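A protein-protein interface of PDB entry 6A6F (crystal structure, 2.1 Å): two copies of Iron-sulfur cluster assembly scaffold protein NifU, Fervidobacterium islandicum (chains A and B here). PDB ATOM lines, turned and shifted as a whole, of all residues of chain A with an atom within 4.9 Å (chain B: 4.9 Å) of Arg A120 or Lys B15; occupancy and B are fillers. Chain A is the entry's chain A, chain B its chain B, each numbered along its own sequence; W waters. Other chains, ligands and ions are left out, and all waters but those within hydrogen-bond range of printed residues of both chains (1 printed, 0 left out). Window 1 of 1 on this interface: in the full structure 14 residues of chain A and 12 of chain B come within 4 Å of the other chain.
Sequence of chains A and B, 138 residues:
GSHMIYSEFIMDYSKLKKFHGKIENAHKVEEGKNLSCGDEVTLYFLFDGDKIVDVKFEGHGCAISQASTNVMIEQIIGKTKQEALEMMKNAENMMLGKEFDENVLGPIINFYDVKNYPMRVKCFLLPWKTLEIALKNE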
ATOM      1  N   ILE A   5     -13.138 -38.208  26.115  1.00  0.00           N
ATOM      2  CA  ILE A   5     -14.459 -37.805  25.629  1.00  0.00           C
ATOM      3  C   ILE A   5     -14.431 -37.311  24.188  1.00  0.00           C
ATOM      4  O   ILE A   5     -15.422 -37.423  23.473  1.00  0.00           O
ATOM      5  CB  ILE A   5     -15.091 -36.754  26.577  1.00  0.00           C
ATOM      6  CG1 ILE A   5     -16.556 -36.533  26.274  1.00  0.00           C
ATOM      7  CG2 ILE A   5     -14.335 -35.430  26.501  1.00  0.00           C
ATOM      8  CD1 ILE A   5     -17.247 -35.625  27.293  1.00  0.00           C
ATOM      9  N   TYR A   6     -13.295 -36.791  23.743  1.00  0.00           N
ATOM     10  CA  TYR A   6     -13.178 -36.229  22.399  1.00  0.00           C
ATOM     11  C   TYR A   6     -12.884 -37.258  21.319  1.00  0.00           C
ATOM     12  O   TYR A   6     -11.746 -37.392  20.923  1.00  0.00           O
ATOM     13  CB  TYR A   6     -12.094 -35.132  22.375  1.00  0.00           C
ATOM     14  CG  TYR A   6     -12.440 -33.953  23.287  1.00  0.00           C
ATOM     15  CD1 TYR A   6     -13.514 -33.118  23.005  1.00  0.00           C
ATOM     16  CD2 TYR A   6     -11.719 -33.714  24.441  1.00  0.00           C
ATOM     17  CE1 TYR A   6     -13.836 -32.059  23.837  1.00  0.00           C
ATOM     18  CE2 TYR A   6     -12.013 -32.648  25.281  1.00  0.00           C
ATOM     19  CZ  TYR A   6     -13.061 -31.818  24.980  1.00  0.00           C
ATOM     20  OH  TYR A   6     -13.364 -30.795  25.829  1.00  0.00           O
ATOM     21  N   CYS A  37     -19.799 -23.502  30.920  1.00  0.00           N
ATOM     22  CA  CYS A  37     -18.681 -23.779  30.006  1.00  0.00           C
ATOM     23  C   CYS A  37     -18.236 -22.561  29.167  1.00  0.00           C
ATOM     24  O   CYS A  37     -17.053 -22.443  28.839  1.00  0.00           O
ATOM     25  CB  CYS A  37     -19.001 -24.990  29.052  1.00  0.00           C
ATOM     26  SG  CYS A  37     -17.661 -25.487  27.922  1.00  0.00           S
ATOM     27  N   CYS A  62     -17.256 -24.950  22.912  1.00  0.00           N
ATOM     28  CA  CYS A  62     -16.438 -26.138  22.933  1.00  0.00           C
ATOM     29  C   CYS A  62     -16.709 -27.129  21.742  1.00  0.00           C
ATOM     30  O   CYS A  62     -17.681 -26.988  20.952  1.00  0.00           O
ATOM     31  CB  CYS A  62     -16.616 -26.821  24.279  1.00  0.00           C
ATOM     32  SG  CYS A  62     -18.124 -27.769  24.559  1.00  0.00           S
ATOM     33  N   ILE A  64     -17.722 -30.229  21.919  1.00  0.00           N
ATOM     34  CA  ILE A  64     -18.897 -31.011  22.154  1.00  0.00           C
ATOM     35  C   ILE A  64     -20.162 -30.230  21.766  1.00  0.00           C
ATOM     36  O   ILE A  64     -21.032 -30.804  21.067  1.00  0.00           O
ATOM     37  CB  ILE A  64     -18.976 -31.492  23.610  1.00  0.00           C
ATOM     38  CG1 ILE A  64     -17.876 -32.524  23.907  1.00  0.00           C
ATOM     39  CG2 ILE A  64     -20.327 -32.118  23.892  1.00  0.00           C
ATOM     40  CD1 ILE A  64     -17.814 -32.911  25.382  1.00  0.00           C
ATOM     41  N   VAL A 114     -21.094 -39.087  26.334  1.00  0.00           N
ATOM     42  CA  VAL A 114     -21.067 -37.810  27.009  1.00  0.00           C
ATOM     43  C   VAL A 114     -21.869 -37.838  28.302  1.00  0.00           C
ATOM     44  O   VAL A 114     -21.585 -37.071  29.241  1.00  0.00           O
ATOM     45  CB  VAL A 114     -21.574 -36.719  26.036  1.00  0.00           C
ATOM     46  CG1 VAL A 114     -21.704 -35.381  26.750  1.00  0.00           C
ATOM     47  CG2 VAL A 114     -20.621 -36.644  24.846  1.00  0.00           C
ATOM     48  N   TYR A 117     -20.372 -37.631  31.694  1.00  0.00           N
ATOM     49  CA  TYR A 117     -19.765 -36.397  32.136  1.00  0.00           C
ATOM     50  C   TYR A 117     -20.861 -35.337  32.355  1.00  0.00           C
ATOM     51  O   TYR A 117     -21.214 -34.581  31.430  1.00  0.00           O
ATOM     52  CB  TYR A 117     -18.744 -35.924  31.129  1.00  0.00           C
ATOM     53  CG  TYR A 117     -17.647 -36.891  30.823  1.00  0.00           C
ATOM     54  CD1 TYR A 117     -16.366 -36.686  31.283  1.00  0.00           C
ATOM     55  CD2 TYR A 117     -17.875 -37.991  29.992  1.00  0.00           C
ATOM     56  CE1 TYR A 117     -15.322 -37.564  30.962  1.00  0.00           C
ATOM     57  CE2 TYR A 117     -16.864 -38.875  29.663  1.00  0.00           C
ATOM     58  CZ  TYR A 117     -15.588 -38.675  30.155  1.00  0.00           C
ATOM     59  OH  TYR A 117     -14.601 -39.566  29.784  1.00  0.00           O
ATOM     60  N   PRO A 118     -21.403 -35.276  33.568  1.00  0.00           N
ATOM     61  CA  PRO A 118     -22.471 -34.350  33.869  1.00  0.00           C
ATOM     62  C   PRO A 118     -22.233 -32.891  33.463  1.00  0.00           C
ATOM     63  O   PRO A 118     -23.170 -32.227  33.072  1.00  0.00           O
ATOM     64  CB  PRO A 118     -22.617 -34.463  35.402  1.00  0.00           C
ATOM     65  CG  PRO A 118     -21.376 -35.150  35.870  1.00  0.00           C
ATOM     66  CD  PRO A 118     -21.034 -36.069  34.756  1.00  0.00           C
ATOM     67  N   MET A 119     -21.027 -32.369  33.560  1.00  0.00           N
ATOM     68  CA  MET A 119     -20.843 -30.988  33.102  1.00  0.00           C
ATOM     69  C   MET A 119     -20.971 -30.855  31.567  1.00  0.00           C
ATOM     70  O   MET A 119     -21.628 -29.911  31.080  1.00  0.00           O
ATOM     71  CB  MET A 119     -19.541 -30.372  33.628  1.00  0.00           C
ATOM     72  CG  MET A 119     -19.759 -29.564  34.909  1.00  0.00           C
ATOM     73  SD  MET A 119     -18.252 -28.718  35.435  1.00  0.00           S
ATOM     74  CE  MET A 119     -17.245 -30.078  36.056  1.00  0.00           C
ATOM     75  N   ARG A 120     -20.435 -31.839  30.834  1.00  0.00           N
ATOM     76  CA  ARG A 120     -20.480 -31.829  29.366  1.00  0.00           C
ATOM     77  C   ARG A 120     -21.849 -32.190  28.774  1.00  0.00           C
ATOM     78  O   ARG A 120     -22.119 -31.916  27.615  1.00  0.00           O
ATOM     79  CB  ARG A 120     -19.382 -32.717  28.784  1.00  0.00           C
ATOM     80  CG  ARG A 120     -18.013 -32.504  29.393  1.00  0.00           C
ATOM     81  CD  ARG A 120     -17.630 -31.014  29.493  1.00  0.00           C
ATOM     82  NE  ARG A 120     -17.503 -30.385  28.189  1.00  0.00           N
ATOM     83  CZ  ARG A 120     -16.423 -30.413  27.436  1.00  0.00           C
ATOM     84  NH1 ARG A 120     -16.446 -29.818  26.262  1.00  0.00           N
ATOM     85  NH2 ARG A 120     -15.333 -31.082  27.816  1.00  0.00           N
ATOM     86  N   VAL A 121     -22.714 -32.782  29.563  1.00  0.00           N
ATOM     87  CA  VAL A 121     -24.068 -33.017  29.157  1.00  0.00           C
ATOM     88  C   VAL A 121     -24.767 -31.730  28.750  1.00  0.00           C
ATOM     89  O   VAL A 121     -25.573 -31.720  27.836  1.00  0.00           O
ATOM     90  CB  VAL A 121     -24.864 -33.710  30.285  1.00  0.00           C
ATOM     91  CG1 VAL A 121     -26.362 -33.682  30.005  1.00  0.00           C
ATOM     92  CG2 VAL A 121     -24.414 -35.148  30.412  1.00  0.00           C
ATOM     93  N   LYS A 122     -24.455 -30.641  29.418  1.00  0.00           N
ATOM     94  CA  LYS A 122     -25.003 -29.348  29.059  1.00  0.00           C
ATOM     95  C   LYS A 122     -24.518 -28.806  27.723  1.00  0.00           C
ATOM     96  O   LYS A 122     -25.252 -28.082  27.086  1.00  0.00           O
ATOM     97  CB  LYS A 122     -24.666 -28.317  30.134  1.00  0.00           C
ATOM     98  CG  LYS A 122     -25.611 -28.405  31.321  1.00  0.00           C
ATOM     99  CD  LYS A 122     -24.991 -29.095  32.522  1.00  0.00           C
ATOM    100  CE  LYS A 122     -25.302 -28.305  33.789  1.00  0.00           C
ATOM    101  NZ  LYS A 122     -24.759 -26.950  33.545  1.00  0.00           N
ATOM    102  N   CYS A 123     -23.272 -29.122  27.363  1.00  0.00           N
ATOM    103  CA  CYS A 123     -22.677 -28.795  26.088  1.00  0.00           C
ATOM    104  C   CYS A 123     -23.389 -29.541  24.951  1.00  0.00           C
ATOM    105  O   CYS A 123     -23.792 -28.936  23.988  1.00  0.00           O
ATOM    106  CB  CYS A 123     -21.166 -29.103  26.091  1.00  0.00           C
ATOM    107  SG  CYS A 123     -20.279 -28.412  27.536  1.00  0.00           S
ATOM    108  N   PHE A 124     -23.539 -30.857  25.090  1.00  0.00           N
ATOM    109  CA  PHE A 124     -24.322 -31.629  24.174  1.00  0.00           C
ATOM    110  C   PHE A 124     -25.755 -31.120  23.989  1.00  0.00           C
ATOM    111  O   PHE A 124     -26.265 -31.046  22.850  1.00  0.00           O
ATOM    112  CB  PHE A 124     -24.433 -33.069  24.639  1.00  0.00           C
ATOM    113  CG  PHE A 124     -25.342 -33.875  23.795  1.00  0.00           C
ATOM    114  CD1 PHE A 124     -25.007 -34.175  22.490  1.00  0.00           C
ATOM    115  CD2 PHE A 124     -26.554 -34.302  24.276  1.00  0.00           C
ATOM    116  CE1 PHE A 124     -25.860 -34.939  21.684  1.00  0.00           C
ATOM    117  CE2 PHE A 124     -27.424 -35.037  23.478  1.00  0.00           C
ATOM    118  CZ  PHE A 124     -27.076 -35.357  22.175  1.00  0.00           C
ATOM    119  N   MET B  11      -6.872 -29.599  24.374  1.00  0.00           N
ATOM    120  CA  MET B  11      -8.297 -29.442  24.719  1.00  0.00           C
ATOM    121  C   MET B  11      -8.535 -28.609  25.978  1.00  0.00           C
ATOM    122  O   MET B  11      -9.490 -27.819  26.004  1.00  0.00           O
ATOM    123  CB  MET B  11      -8.971 -30.809  24.771  1.00  0.00           C
ATOM    124  CG  MET B  11      -8.832 -31.544  23.451  1.00  0.00           C
ATOM    125  SD  MET B  11      -9.294 -30.647  21.918  1.00  0.00           S
ATOM    126  CE  MET B  11     -11.004 -30.265  22.342  1.00  0.00           C
ATOM    127  N   ASP B  12      -7.681 -28.725  27.006  1.00  0.00           N
ATOM    128  CA  ASP B  12      -7.795 -27.833  28.150  1.00  0.00           C
ATOM    129  C   ASP B  12      -7.643 -26.383  27.718  1.00  0.00           C
ATOM    130  O   ASP B  12      -8.511 -25.570  27.987  1.00  0.00           O
ATOM    131  CB  ASP B  12      -6.813 -28.145  29.310  1.00  0.00           C
ATOM    132  CG  ASP B  12      -7.134 -29.458  30.078  1.00  0.00           C
ATOM    133  OD1 ASP B  12      -8.318 -29.898  30.108  1.00  0.00           O
ATOM    134  OD2 ASP B  12      -6.179 -30.048  30.684  1.00  0.00           O
ATOM    135  N   TYR B  13      -6.541 -26.055  27.074  1.00  0.00           N
ATOM    136  CA  TYR B  13      -6.270 -24.662  26.685  1.00  0.00           C
ATOM    137  C   TYR B  13      -7.239 -24.094  25.625  1.00  0.00           C
ATOM    138  O   TYR B  13      -7.419 -22.876  25.519  1.00  0.00           O
ATOM    139  CB  TYR B  13      -4.818 -24.460  26.249  1.00  0.00           C
ATOM    140  CG  TYR B  13      -3.949 -24.117  27.389  1.00  0.00           C
ATOM    141  CD1 TYR B  13      -4.009 -22.857  27.972  1.00  0.00           C
ATOM    142  CD2 TYR B  13      -3.141 -25.092  27.975  1.00  0.00           C
ATOM    143  CE1 TYR B  13      -3.239 -22.555  29.058  1.00  0.00           C
ATOM    144  CE2 TYR B  13      -2.362 -24.799  29.068  1.00  0.00           C
ATOM    145  CZ  TYR B  13      -2.409 -23.529  29.599  1.00  0.00           C
ATOM    146  OH  TYR B  13      -1.624 -23.244  30.650  1.00  0.00           O
ATOM    147  N   SER B  14      -7.848 -24.977  24.846  1.00  0.00           N
ATOM    148  CA  SER B  14      -8.805 -24.569  23.812  1.00  0.00           C
ATOM    149  C   SER B  14     -10.073 -23.986  24.433  1.00  0.00           C
ATOM    150  O   SER B  14     -10.674 -23.121  23.883  1.00  0.00           O
ATOM    151  CB  SER B  14      -9.235 -25.779  22.981  1.00  0.00           C
ATOM    152  OG  SER B  14     -10.047 -25.354  21.890  1.00  0.00           O
ATOM    153  N   LYS B  15     -10.496 -24.569  25.532  1.00  0.00           N
ATOM    154  CA  LYS B  15     -11.680 -24.161  26.260  1.00  0.00           C
ATOM    155  C   LYS B  15     -11.468 -22.998  27.263  1.00  0.00           C
ATOM    156  O   LYS B  15     -12.443 -22.446  27.755  1.00  0.00           O
ATOM    157  CB  LYS B  15     -12.184 -25.343  27.094  1.00  0.00           C
ATOM    158  CG  LYS B  15     -12.724 -26.475  26.296  1.00  0.00           C
ATOM    159  CD  LYS B  15     -13.582 -27.365  27.219  1.00  0.00           C
ATOM    160  CE  LYS B  15     -12.753 -28.164  28.203  1.00  0.00           C
ATOM    161  NZ  LYS B  15     -11.727 -28.946  27.452  1.00  0.00           N
ATOM    162  N   LEU B  16     -10.231 -22.631  27.567  1.00  0.00           N
ATOM    163  CA  LEU B  16      -9.968 -21.488  28.460  1.00  0.00           C
ATOM    164  C   LEU B  16     -10.637 -20.197  27.941  1.00  0.00           C
ATOM    165  O   LEU B  16     -10.537 -19.859  26.757  1.00  0.00           O
ATOM    166  CB  LEU B  16      -8.467 -21.300  28.595  1.00  0.00           C
ATOM    167  CG  LEU B  16      -7.923 -20.370  29.658  1.00  0.00           C
ATOM    168  CD1 LEU B  16      -8.353 -20.908  31.017  1.00  0.00           C
ATOM    169  CD2 LEU B  16      -6.404 -20.260  29.527  1.00  0.00           C
ATOM    170  N   LYS B  17     -11.366 -19.517  28.819  1.00  0.00           N
ATOM    171  CA  LYS B  17     -12.106 -18.310  28.438  1.00  0.00           C
ATOM    172  C   LYS B  17     -11.536 -17.058  29.030  1.00  0.00           C
ATOM    173  O   LYS B  17     -11.987 -15.995  28.670  1.00  0.00           O
ATOM    174  CB  LYS B  17     -13.615 -18.385  28.824  1.00  0.00           C
ATOM    175  CG  LYS B  17     -14.356 -19.648  28.338  1.00  0.00           C
ATOM    176  CD  LYS B  17     -14.375 -19.835  26.823  1.00  0.00           C
ATOM    177  CE  LYS B  17     -15.560 -19.129  26.183  1.00  0.00           C
ATOM    178  NZ  LYS B  17     -15.170 -18.490  24.910  1.00  0.00           N
HETATM  179  O   HOH W   1     -14.671 -23.419  28.916  1.00  0.00           O
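Among the printed residues, merely in contact across the chains: Tyr A6 with Met B11 (3.6 Å), Arg A120 with Lys B15 (3.9 Å) and Cys A37 with Lys B17 (3.9 Å).
Of the 14 printed residues of chain A, 3 touch a printed residue of chain B. Printed residues of chain A that touch a printed residue of chain B: Tyr A6, Cys A37 and Arg A120. Hydrophobic or aromatic side chains of chain B within 4 Å of the printed part of chain A: Met B11. Among the printed residues, no Asp or Glu carboxylate lies within 4 Å of a Lys or Arg side-chain nitrogen of the other chain.
The side-chain amino group (NZ) of Lys B15 lies within hydrogen-bond range of the side-chain hydroxyl (OH) of Tyr A6 (3.0 Å).
OH of Tyr A6 lies within hydrogen-bond range of NH2 of Arg A120, 2.8 Å away. SG of Cys A62 lies close to NH1 of Arg A120, 3.1 Å away. NE of Arg A120 lies close to SG of Cys A123 (3.5 Å). The side-chain amino group (NZ) of Lys B15 lies within hydrogen-bond range of the backbone carbonyl oxygen (O) of Met B11 (2.9 Å).
No position is printed for both chains. Of the 4 pairs that touch across the chains among the printed residues, none has its exchanged pair printed and touching as well.
Water W1 bridges O of Cys A37 (2.6 Å) and O of Lys B15 (2.7 Å).
Printed residues of chain B within 4 Å of Arg A120: Lys B15 (3.9 Å). Of the printed residues of chain A, Lys B17 touches Cys A37. Of the printed residues of chain B, Cys A37 touches Lys B17 (3.9 Å). Of the printed residues of chain B, Tyr A6 touches Met B11 (3.6 Å) and Lys B15 (3.0 Å). Of the printed residues of chain A, Met B11 touches Tyr A6. Val A121 touches none of the printed residues of chain B. Ile A64 touches none of the printed residues of chain B. The nearest residue of chain A that does not touch Lys B15 is Cys A62 (4.3 Å). The nearest printed residue of chain A that does not touch Lys B17 is Cys A62 (6.9 Å).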
